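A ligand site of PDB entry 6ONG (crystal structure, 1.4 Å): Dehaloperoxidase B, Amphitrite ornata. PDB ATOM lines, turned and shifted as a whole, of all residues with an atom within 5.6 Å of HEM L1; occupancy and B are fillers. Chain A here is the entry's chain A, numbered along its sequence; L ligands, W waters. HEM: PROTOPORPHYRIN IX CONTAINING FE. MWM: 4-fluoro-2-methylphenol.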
ATOM      1  N   PHE A  24     -28.921   1.532  14.748  1.00  0.00           N
ATOM      2  CA  PHE A  24     -29.630   1.408  13.453  1.00  0.00           C
ATOM      3  C   PHE A  24     -31.106   1.129  13.707  1.00  0.00           C
ATOM      4  O   PHE A  24     -31.956   1.824  13.170  1.00  0.00           O
ATOM      5  CB  PHE A  24     -28.950   0.343  12.610  1.00  0.00           C
ATOM      6  CG  PHE A  24     -29.767  -0.202  11.465  1.00  0.00           C
ATOM      7  CD1 PHE A  24     -29.949   0.551  10.303  1.00  0.00           C
ATOM      8  CD2 PHE A  24     -30.307  -1.480  11.529  1.00  0.00           C
ATOM      9  CE1 PHE A  24     -30.638   0.004   9.236  1.00  0.00           C
ATOM     10  CE2 PHE A  24     -30.989  -2.019  10.461  1.00  0.00           C
ATOM     11  CZ  PHE A  24     -31.170  -1.264   9.321  1.00  0.00           C
ATOM     12  N   GLU A  31     -37.191  -0.515   9.896  1.00  0.00           N
ATOM     13  CA  GLU A  31     -36.260  -1.553   9.399  1.00  0.00           C
ATOM     14  C   GLU A  31     -36.535  -2.896  10.088  1.00  0.00           C
ATOM     15  O   GLU A  31     -36.019  -3.913   9.606  1.00  0.00           O
ATOM     16  CB  GLU A  31     -34.819  -1.071   9.500  1.00  0.00           C
ATOM     17  CG  GLU A  31     -34.488   0.035   8.514  1.00  0.00           C
ATOM     18  CD  GLU A  31     -34.377  -0.401   7.060  1.00  0.00           C
ATOM     19  OE1 GLU A  31     -35.116   0.102   6.211  1.00  0.00           O
ATOM     20  OE2 GLU A  31     -33.611  -1.307   6.805  1.00  0.00           O
ATOM     21  N   ASN A  34     -37.759  -6.419   8.385  1.00  0.00           N
ATOM     22  CA  ASN A  34     -36.843  -7.548   8.041  1.00  0.00           C
ATOM     23  C   ASN A  34     -36.368  -8.309   9.281  1.00  0.00           C
ATOM     24  O   ASN A  34     -35.658  -9.315   9.088  1.00  0.00           O
ATOM     25  CB  ASN A  34     -35.614  -7.067   7.264  1.00  0.00           C
ATOM     26  CG  ASN A  34     -35.922  -6.654   5.839  1.00  0.00           C
ATOM     27  OD1 ASN A  34     -36.586  -7.395   5.114  1.00  0.00           O
ATOM     28  ND2 ASN A  34     -35.420  -5.505   5.420  1.00  0.00           N
ATOM     29  N   PHE A  35     -36.758  -7.893  10.502  1.00  0.00           N
ATOM     30  CA  PHE A  35     -36.337  -8.477  11.803  1.00  0.00           C
ATOM     31  C   PHE A  35     -37.571  -8.595  12.730  1.00  0.00           C
ATOM     32  O   PHE A  35     -37.569  -8.029  13.838  1.00  0.00           O
ATOM     33  CB  PHE A  35     -35.252  -7.607  12.434  1.00  0.00           C
ATOM     34  CG  PHE A  35     -34.025  -7.377  11.579  1.00  0.00           C
ATOM     35  CD1 PHE A  35     -33.091  -8.384  11.403  1.00  0.00           C
ATOM     36  CD2 PHE A  35     -33.825  -6.179  10.910  1.00  0.00           C
ATOM     37  CE1 PHE A  35     -31.970  -8.186  10.608  1.00  0.00           C
ATOM     38  CE2 PHE A  35     -32.711  -5.988  10.116  1.00  0.00           C
ATOM     39  CZ  PHE A  35     -31.789  -6.994   9.959  1.00  0.00           C
ATOM     40  N   TYR A  38     -37.436  -9.129  16.507  1.00  0.00           N
ATOM     41  CA  TYR A  38     -36.838  -8.082  17.367  1.00  0.00           C
ATOM     42  C   TYR A  38     -37.917  -7.052  17.783  1.00  0.00           C
ATOM     43  O   TYR A  38     -37.618  -6.136  18.571  1.00  0.00           O
ATOM     44  CB  TYR A  38     -35.560  -7.525  16.721  1.00  0.00           C
ATOM     45  CG  TYR A  38     -34.470  -8.541  16.428  1.00  0.00           C
ATOM     46  CD1 TYR A  38     -34.432  -9.754  17.102  1.00  0.00           C
ATOM     47  CD2 TYR A  38     -33.452  -8.292  15.506  1.00  0.00           C
ATOM     48  CE1 TYR A  38     -33.461 -10.701  16.852  1.00  0.00           C
ATOM     49  CE2 TYR A  38     -32.477  -9.250  15.217  1.00  0.00           C
ATOM     50  CZ  TYR A  38     -32.496 -10.469  15.886  1.00  0.00           C
ATOM     51  OH  TYR A  38     -31.559 -11.449  15.653  1.00  0.00           O
ATOM     52  N   LYS A  51     -29.862 -15.245  18.951  1.00  0.00           N
ATOM     53  CA  LYS A  51     -29.564 -15.016  17.513  1.00  0.00           C
ATOM     54  C   LYS A  51     -29.256 -13.529  17.309  1.00  0.00           C
ATOM     55  O   LYS A  51     -28.561 -13.172  16.357  1.00  0.00           O
ATOM     56  CB  LYS A  51     -30.714 -15.422  16.597  1.00  0.00           C
ATOM     57  CG  LYS A  51     -31.004 -16.917  16.556  1.00  0.00           C
ATOM     58  CD  LYS A  51     -32.168 -17.269  15.656  1.00  0.00           C
ATOM     59  CE  LYS A  51     -32.376 -18.767  15.553  1.00  0.00           C
ATOM     60  NZ  LYS A  51     -33.466 -19.096  14.609  1.00  0.00           N
ATOM     61  N   ASP A  54     -25.525 -13.512  18.177  1.00  0.00           N
ATOM     62  CA  ASP A  54     -24.774 -14.413  17.257  1.00  0.00           C
ATOM     63  C   ASP A  54     -24.779 -13.818  15.846  1.00  0.00           C
ATOM     64  O   ASP A  54     -23.700 -13.664  15.255  1.00  0.00           O
ATOM     65  CB  ASP A  54     -25.341 -15.835  17.206  1.00  0.00           C
ATOM     66  CG  ASP A  54     -24.448 -16.801  16.444  1.00  0.00           C
ATOM     67  OD1 ASP A  54     -23.322 -17.064  16.928  1.00  0.00           O
ATOM     68  OD2 ASP A  54     -24.845 -17.231  15.338  1.00  0.00           O
ATOM     69  N   HIS A  55     -25.946 -13.503  15.312  1.00  0.00           N
ATOM     70  CA  HIS A  55     -26.053 -13.016  13.919  1.00  0.00           C
ATOM     71  C   HIS A  55     -25.380 -11.657  13.827  1.00  0.00           C
ATOM     72  O   HIS A  55     -24.683 -11.377  12.831  1.00  0.00           O
ATOM     73  CB  HIS A  55     -27.496 -13.000  13.434  1.00  0.00           C
ATOM     74  CG  HIS A  55     -28.101 -14.358  13.341  1.00  0.00           C
ATOM     75  ND1 HIS A  55     -29.207 -14.591  12.566  1.00  0.00           N
ATOM     76  CD2 HIS A  55     -27.774 -15.546  13.903  1.00  0.00           C
ATOM     77  CE1 HIS A  55     -29.539 -15.859  12.624  1.00  0.00           C
ATOM     78  NE2 HIS A  55     -28.679 -16.469  13.448  1.00  0.00           N
ATOM     79  N   LYS A  58     -21.669 -12.114  13.711  1.00  0.00           N
ATOM     80  CA  LYS A  58     -21.247 -12.678  12.409  1.00  0.00           C
ATOM     81  C   LYS A  58     -21.347 -11.628  11.296  1.00  0.00           C
ATOM     82  O   LYS A  58     -20.422 -11.557  10.426  1.00  0.00           O
ATOM     83  CB  LYS A  58     -22.030 -13.941  12.097  1.00  0.00           C
ATOM     84  CG  LYS A  58     -21.495 -15.149  12.852  1.00  0.00           C
ATOM     85  CD  LYS A  58     -22.457 -16.288  12.815  1.00  0.00           C
ATOM     86  CE  LYS A  58     -21.943 -17.547  13.483  1.00  0.00           C
ATOM     87  NZ  LYS A  58     -23.022 -18.570  13.537  1.00  0.00           N
ATOM     88  N   VAL A  59     -22.344 -10.768  11.323  1.00  0.00           N
ATOM     89  CA  VAL A  59     -22.456  -9.653  10.360  1.00  0.00           C
ATOM     90  C   VAL A  59     -21.221  -8.767  10.491  1.00  0.00           C
ATOM     91  O   VAL A  59     -20.601  -8.456   9.455  1.00  0.00           O
ATOM     92  CB  VAL A  59     -23.761  -8.878  10.591  1.00  0.00           C
ATOM     93  CG1 VAL A  59     -23.768  -7.562   9.833  1.00  0.00           C
ATOM     94  CG2 VAL A  59     -24.951  -9.718  10.211  1.00  0.00           C
ATOM     95  N   PHE A  60     -20.879  -8.360  11.716  1.00  0.00           N
ATOM     96  CA  PHE A  60     -19.770  -7.399  11.885  1.00  0.00           C
ATOM     97  C   PHE A  60     -18.420  -8.094  11.654  1.00  0.00           C
ATOM     98  O   PHE A  60     -17.477  -7.461  11.173  1.00  0.00           O
ATOM     99  CB  PHE A  60     -19.847  -6.670  13.225  1.00  0.00           C
ATOM    100  CG  PHE A  60     -20.771  -5.487  13.113  1.00  0.00           C
ATOM    101  CD1 PHE A  60     -22.149  -5.677  13.024  1.00  0.00           C
ATOM    102  CD2 PHE A  60     -20.257  -4.206  13.028  1.00  0.00           C
ATOM    103  CE1 PHE A  60     -22.992  -4.577  12.909  1.00  0.00           C
ATOM    104  CE2 PHE A  60     -21.118  -3.113  12.934  1.00  0.00           C
ATOM    105  CZ  PHE A  60     -22.482  -3.313  12.854  1.00  0.00           C
ATOM    106  N   LEU A  62     -17.889 -10.230   9.316  1.00  0.00           N
ATOM    107  CA  LEU A  62     -17.684 -10.191   7.855  1.00  0.00           C
ATOM    108  C   LEU A  62     -17.512  -8.740   7.415  1.00  0.00           C
ATOM    109  O   LEU A  62     -16.682  -8.468   6.548  1.00  0.00           O
ATOM    110  CB  LEU A  62     -18.830 -10.910   7.121  1.00  0.00           C
ATOM    111  CG  LEU A  62     -18.746 -10.928   5.590  1.00  0.00           C
ATOM    112  CD1 LEU A  62     -17.424 -11.505   5.086  1.00  0.00           C
ATOM    113  CD2 LEU A  62     -19.913 -11.717   5.021  1.00  0.00           C
ATOM    114  N   MET A  63     -18.240  -7.803   8.003  1.00  0.00           N
ATOM    115  CA  MET A  63     -18.100  -6.395   7.608  1.00  0.00           C
ATOM    116  C   MET A  63     -16.660  -5.927   7.842  1.00  0.00           C
ATOM    117  O   MET A  63     -16.095  -5.218   6.981  1.00  0.00           O
ATOM    118  CB  MET A  63     -19.054  -5.494   8.392  1.00  0.00           C
ATOM    119  CG  MET A  63     -19.028  -4.045   7.917  1.00  0.00           C
ATOM    120  SD  MET A  63     -19.684  -2.866   9.119  1.00  0.00           S
ATOM    121  CE  MET A  63     -21.411  -3.350   9.132  1.00  0.00           C
ATOM    122  N   VAL A  66     -14.531  -7.225   5.038  1.00  0.00           N
ATOM    123  CA  VAL A  66     -14.767  -6.487   3.772  1.00  0.00           C
ATOM    124  C   VAL A  66     -14.051  -5.128   3.867  1.00  0.00           C
ATOM    125  O   VAL A  66     -13.384  -4.707   2.922  1.00  0.00           O
ATOM    126  CB  VAL A  66     -16.278  -6.329   3.522  1.00  0.00           C
ATOM    127  CG1 VAL A  66     -16.546  -5.414   2.347  1.00  0.00           C
ATOM    128  CG2 VAL A  66     -16.897  -7.710   3.320  1.00  0.00           C
ATOM    129  N   LEU A  83     -22.196 -10.392  -1.002  1.00  0.00           N
ATOM    130  CA  LEU A  83     -23.258  -9.751  -0.190  1.00  0.00           C
ATOM    131  C   LEU A  83     -24.570  -9.667  -0.986  1.00  0.00           C
ATOM    132  O   LEU A  83     -25.650  -9.751  -0.381  1.00  0.00           O
ATOM    133  CB  LEU A  83     -22.792  -8.376   0.276  1.00  0.00           C
ATOM    134  CG  LEU A  83     -21.673  -8.370   1.312  1.00  0.00           C
ATOM    135  CD1 LEU A  83     -21.182  -6.959   1.527  1.00  0.00           C
ATOM    136  CD2 LEU A  83     -22.095  -8.992   2.640  1.00  0.00           C
ATOM    137  N   MET A  86     -25.923 -13.697  -1.341  1.00  0.00           N
ATOM    138  CA  MET A  86     -26.311 -14.401  -0.090  1.00  0.00           C
ATOM    139  C   MET A  86     -27.831 -14.592  -0.053  1.00  0.00           C
ATOM    140  O   MET A  86     -28.565 -13.596  -0.232  1.00  0.00           O
ATOM    141  CB  MET A  86     -25.910 -13.569   1.128  1.00  0.00           C
ATOM    142  CG  MET A  86     -24.483 -13.735   1.516  1.00  0.00           C
ATOM    143  SD  MET A  86     -24.088 -12.543   2.794  1.00  0.00           S
ATOM    144  CE  MET A  86     -25.139 -13.122   4.125  1.00  0.00           C
ATOM    145  N   GLN A  88     -29.642 -14.986   2.427  1.00  0.00           N
ATOM    146  CA  GLN A  88     -30.080 -14.218   3.616  1.00  0.00           C
ATOM    147  C   GLN A  88     -30.406 -12.774   3.224  1.00  0.00           C
ATOM    148  O   GLN A  88     -31.140 -12.121   3.955  1.00  0.00           O
ATOM    149  CB  GLN A  88     -29.006 -14.299   4.690  1.00  0.00           C
ATOM    150  CG  GLN A  88     -28.641 -15.722   5.086  1.00  0.00           C
ATOM    151  CD  GLN A  88     -27.385 -16.248   4.422  1.00  0.00           C
ATOM    152  OE1 GLN A  88     -27.132 -16.037   3.242  1.00  0.00           O
ATOM    153  NE2 GLN A  88     -26.588 -16.959   5.192  1.00  0.00           N
ATOM    154  N   HIS A  89     -29.845 -12.309   2.107  1.00  0.00           N
ATOM    155  CA  HIS A  89     -29.991 -10.922   1.593  1.00  0.00           C
ATOM    156  C   HIS A  89     -30.983 -10.846   0.434  1.00  0.00           C
ATOM    157  O   HIS A  89     -31.079  -9.782  -0.167  1.00  0.00           O
ATOM    158  CB  HIS A  89     -28.630 -10.363   1.181  1.00  0.00           C
ATOM    159  CG  HIS A  89     -27.773 -10.070   2.353  1.00  0.00           C
ATOM    160  ND1 HIS A  89     -26.455  -9.700   2.223  1.00  0.00           N
ATOM    161  CD2 HIS A  89     -28.014 -10.132   3.675  1.00  0.00           C
ATOM    162  CE1 HIS A  89     -25.933  -9.506   3.412  1.00  0.00           C
ATOM    163  NE2 HIS A  89     -26.857  -9.756   4.319  1.00  0.00           N
ATOM    164  N   LEU A  92     -33.362  -7.697   0.315  1.00  0.00           N
ATOM    165  CA  LEU A  92     -32.757  -6.391   0.686  1.00  0.00           C
ATOM    166  C   LEU A  92     -32.586  -5.470  -0.531  1.00  0.00           C
ATOM    167  O   LEU A  92     -32.509  -5.949  -1.665  1.00  0.00           O
ATOM    168  CB  LEU A  92     -31.415  -6.614   1.373  1.00  0.00           C
ATOM    169  CG  LEU A  92     -31.444  -7.518   2.606  1.00  0.00           C
ATOM    170  CD1 LEU A  92     -30.133  -7.424   3.364  1.00  0.00           C
ATOM    171  CD2 LEU A  92     -32.625  -7.181   3.521  1.00  0.00           C
ATOM    172  N   ASN A  96     -31.217  -0.337   2.644  1.00  0.00           N
ATOM    173  CA  ASN A  96     -31.041  -1.061   3.930  1.00  0.00           C
ATOM    174  C   ASN A  96     -29.591  -0.847   4.401  1.00  0.00           C
ATOM    175  O   ASN A  96     -29.323  -0.532   5.576  1.00  0.00           O
ATOM    176  CB  ASN A  96     -31.356  -2.550   3.809  1.00  0.00           C
ATOM    177  CG  ASN A  96     -32.783  -2.898   3.432  1.00  0.00           C
ATOM    178  OD1 ASN A  96     -33.012  -3.582   2.432  1.00  0.00           O
ATOM    179  ND2 ASN A  96     -33.733  -2.459   4.238  1.00  0.00           N
ATOM    180  N   PHE A  97     -28.655  -0.983   3.460  1.00  0.00           N
ATOM    181  CA  PHE A  97     -27.204  -0.793   3.735  1.00  0.00           C
ATOM    182  C   PHE A  97     -26.883   0.689   3.988  1.00  0.00           C
ATOM    183  O   PHE A  97     -26.131   0.981   4.895  1.00  0.00           O
ATOM    184  CB  PHE A  97     -26.367  -1.374   2.590  1.00  0.00           C
ATOM    185  CG  PHE A  97     -26.400  -2.877   2.534  1.00  0.00           C
ATOM    186  CD1 PHE A  97     -27.481  -3.562   1.991  1.00  0.00           C
ATOM    187  CD2 PHE A  97     -25.362  -3.626   3.067  1.00  0.00           C
ATOM    188  CE1 PHE A  97     -27.506  -4.948   1.964  1.00  0.00           C
ATOM    189  CE2 PHE A  97     -25.377  -5.009   3.031  1.00  0.00           C
ATOM    190  CZ  PHE A  97     -26.453  -5.673   2.480  1.00  0.00           C
ATOM    191  N   LEU A 100     -27.834   1.481   7.545  1.00  0.00           N
ATOM    192  CA  LEU A 100     -26.907   0.869   8.519  1.00  0.00           C
ATOM    193  C   LEU A 100     -25.667   1.755   8.663  1.00  0.00           C
ATOM    194  O   LEU A 100     -25.272   2.016   9.778  1.00  0.00           O
ATOM    195  CB  LEU A 100     -26.558  -0.541   8.074  1.00  0.00           C
ATOM    196  CG  LEU A 100     -25.559  -1.252   8.980  1.00  0.00           C
ATOM    197  CD1 LEU A 100     -26.107  -1.419  10.398  1.00  0.00           C
ATOM    198  CD2 LEU A 100     -25.192  -2.588   8.378  1.00  0.00           C
ATOM    199  N   PHE A 101     -25.120   2.218   7.543  1.00  0.00           N
ATOM    200  CA  PHE A 101     -23.889   3.044   7.551  1.00  0.00           C
ATOM    201  C   PHE A 101     -24.182   4.449   8.075  1.00  0.00           C
ATOM    202  O   PHE A 101     -23.300   4.973   8.766  1.00  0.00           O
ATOM    203  CB  PHE A 101     -23.134   2.961   6.225  1.00  0.00           C
ATOM    204  CG  PHE A 101     -22.347   1.665   6.171  1.00  0.00           C
ATOM    205  CD1 PHE A 101     -21.108   1.531   6.793  1.00  0.00           C
ATOM    206  CD2 PHE A 101     -22.906   0.536   5.605  1.00  0.00           C
ATOM    207  CE1 PHE A 101     -20.456   0.309   6.809  1.00  0.00           C
ATOM    208  CE2 PHE A 101     -22.250  -0.688   5.635  1.00  0.00           C
ATOM    209  CZ  PHE A 101     -21.015  -0.787   6.216  1.00  0.00           C
ATOM    210  N   LEU A 127     -19.597   0.925  -0.678  1.00  0.00           N
ATOM    211  CA  LEU A 127     -20.190  -0.422  -0.588  1.00  0.00           C
ATOM    212  C   LEU A 127     -21.552  -0.385  -1.298  1.00  0.00           C
ATOM    213  O   LEU A 127     -21.817  -1.301  -2.074  1.00  0.00           O
ATOM    214  CB  LEU A 127     -20.314  -0.876   0.852  1.00  0.00           C
ATOM    215  CG  LEU A 127     -20.948  -2.255   1.012  1.00  0.00           C
ATOM    216  CD1 LEU A 127     -20.125  -3.321   0.309  1.00  0.00           C
ATOM    217  CD2 LEU A 127     -21.115  -2.562   2.485  1.00  0.00           C
HETATM  218  CHA HEM L   1     -27.675 -12.473   7.617  1.00  0.00           C
HETATM  219  CHB HEM L   1     -23.349 -10.132   6.588  1.00  0.00           C
HETATM  220  CHC HEM L   1     -25.785  -5.974   6.024  1.00  0.00           C
HETATM  221  CHD HEM L   1     -29.976  -8.377   6.699  1.00  0.00           C
HETATM  222  C1A HEM L   1     -26.272 -12.115   7.452  1.00  0.00           C
HETATM  223  C2A HEM L   1     -25.185 -13.016   7.749  1.00  0.00           C
HETATM  224  C3A HEM L   1     -23.997 -12.391   7.480  1.00  0.00           C
HETATM  225  C4A HEM L   1     -24.285 -11.104   6.988  1.00  0.00           C
HETATM  226  CMA HEM L   1     -22.603 -12.939   7.656  1.00  0.00           C
HETATM  227  CAA HEM L   1     -25.297 -14.419   8.359  1.00  0.00           C
HETATM  228  CBA HEM L   1     -25.582 -14.328   9.871  1.00  0.00           C
HETATM  229  CGA HEM L   1     -25.876 -15.647  10.530  1.00  0.00           C
HETATM  230  O1A HEM L   1     -25.410 -15.923  11.633  1.00  0.00           O
HETATM  231  O2A HEM L   1     -26.641 -16.457   9.966  1.00  0.00           O
HETATM  232  C1B HEM L   1     -23.654  -8.774   6.323  1.00  0.00           C
HETATM  233  C2B HEM L   1     -22.663  -7.736   6.164  1.00  0.00           C
HETATM  234  C3B HEM L   1     -23.333  -6.564   6.016  1.00  0.00           C
HETATM  235  C4B HEM L   1     -24.752  -6.897   6.106  1.00  0.00           C
HETATM  236  CMB HEM L   1     -21.181  -7.963   6.196  1.00  0.00           C
HETATM  237  CAB HEM L   1     -22.836  -5.195   5.757  1.00  0.00           C
HETATM  238  CBB HEM L   1     -21.628  -4.911   5.239  1.00  0.00           C
HETATM  239  C1C HEM L   1     -27.122  -6.253   6.197  1.00  0.00           C
HETATM  240  C2C HEM L   1     -28.175  -5.292   6.228  1.00  0.00           C
HETATM  241  C3C HEM L   1     -29.360  -5.972   6.432  1.00  0.00           C
HETATM  242  C4C HEM L   1     -29.057  -7.351   6.510  1.00  0.00           C
HETATM  243  CMC HEM L   1     -27.994  -3.800   6.049  1.00  0.00           C
HETATM  244  CAC HEM L   1     -30.720  -5.398   6.612  1.00  0.00           C
HETATM  245  CBC HEM L   1     -30.954  -4.165   7.052  1.00  0.00           C
HETATM  246  C1D HEM L   1     -29.583  -9.684   6.992  1.00  0.00           C
HETATM  247  C2D HEM L   1     -30.664 -10.627   7.389  1.00  0.00           C
HETATM  248  C3D HEM L   1     -30.044 -11.790   7.643  1.00  0.00           C
HETATM  249  C4D HEM L   1     -28.611 -11.511   7.410  1.00  0.00           C
HETATM  250  CMD HEM L   1     -32.161 -10.370   7.453  1.00  0.00           C
HETATM  251  CAD HEM L   1     -30.713 -13.118   8.057  1.00  0.00           C
HETATM  252  CBD HEM L   1     -31.612 -13.010   9.289  1.00  0.00           C
HETATM  253  CGD HEM L   1     -30.690 -13.037  10.459  1.00  0.00           C
HETATM  254  O1D HEM L   1     -29.490 -13.400  10.265  1.00  0.00           O
HETATM  255  O2D HEM L   1     -31.121 -12.724  11.588  1.00  0.00           O
HETATM  256  NA  HEM L   1     -25.656 -10.946   6.946  1.00  0.00           N
HETATM  257  NB  HEM L   1     -24.879  -8.226   6.272  1.00  0.00           N
HETATM  258  NC  HEM L   1     -27.681  -7.490   6.396  1.00  0.00           N
HETATM  259  ND  HEM L   1     -28.300 -10.206   7.027  1.00  0.00           N
HETATM  260 FE   HEM L   1     -26.701  -9.304   6.418  1.00  0.00          FE
HETATM  261  C1  MWM L   2     -28.740  -9.943  10.633  1.00  0.00           C
HETATM  262  C2  MWM L   2     -28.123  -8.607  10.936  1.00  0.00           C
HETATM  263  C3  MWM L   2     -27.721  -8.292  12.224  1.00  0.00           C
HETATM  264  C4  MWM L   2     -27.102  -7.080  12.517  1.00  0.00           C
HETATM  265  C5  MWM L   2     -26.947  -6.130  11.523  1.00  0.00           C
HETATM  266  C6  MWM L   2     -27.366  -6.427  10.256  1.00  0.00           C
HETATM  267  C7  MWM L   2     -27.956  -7.642   9.939  1.00  0.00           C
HETATM  268  F1  MWM L   2     -27.209  -5.487   9.291  1.00  0.00           F
HETATM  269  O1  MWM L   2     -27.885  -9.256  13.175  1.00  0.00           O
HETATM  270  O   HOH W   1     -34.351  -3.913   7.483  1.00  0.00           O
HETATM  271  O   HOH W   2     -34.594 -11.578  10.052  1.00  0.00           O
HETATM  272  O   HOH W   3     -30.238 -10.949  13.434  1.00  0.00           O
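A ring nitrogen (ND1) of His 55 lies within hydrogen-bond range of an oxygen (O1D) of HEM L1. A ring nitrogen (NE2) of His 89 is bound to an iron atom (FE) of HEM L1, 2.2 Å away.
ND1 of His 89 lies within hydrogen-bond range of O of Leu 83 (2.7 Å). ND1 of His 89 sits close to SD of Met 86 (3.7 Å). ND2 of Asn 96 sits at hydrogen-bond distance from OE2 of Glu 31, 2.8 Å away. The side-chain amino group of Lys 58 is in salt-bridge range of the side-chain carboxylate of Asp 54.
Phe 24 touches HEM L1. Glu 31 touches HEM L1. Phe 35 touches HEM L1. Asp 54 touches HEM L1 (OD2 to O1A, 3.97 Å). Lys 58 touches HEM L1. O of Val 59 touches CMB of HEM L1, 3.3 Å away. Leu 62 touches HEM L1 (CB to CMB, 3.9 Å). N of Met 63 touches CMB of HEM L1 (3.5 Å). Leu 83 touches HEM L1 (CD2 to C2B, 3.8 Å). CE of Met 86 touches NA of HEM L1, 3.6 Å away. CB of Gln 88 touches CHA of HEM L1 (3.7 Å). Leu 92 touches HEM L1 (CD1 to C4C, 3.3 Å). Asn 96 touches HEM L1. CE2 of Phe 97 touches CHC of HEM L1, at 3.2 Å. CD2 of Leu 100 touches CMC of HEM L1, 3.8 Å away. Leu 127 touches HEM L1. Hydrophobic or aromatic side chains within 4 Å of HEM L1: Phe 24, Phe 35, His 55, Val 59, Leu 62, Met 63, Leu 83, Met 86, His 89, Leu 92, Phe 97, Leu 100 and Leu 127. Within 4 Å of HEM L1: Phe 24, Glu 31, Phe 35, Asp 54, His 55, Lys 58, Val 59, Leu 62, Met 63, Leu 83, Met 86, Gln 88, His 89, Leu 92, Asn 96, Phe 97, Leu 100 and Leu 127.
Water W3 lies within hydrogen-bond range of OH of Tyr 38, O2D of HEM L1 and O1 of MWM L2. Water W1 lies within hydrogen-bond range of the backbone carbonyl oxygen of Glu 31 (2.7 Å) and the side-chain amide nitrogen of Asn 34 (2.8 Å).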
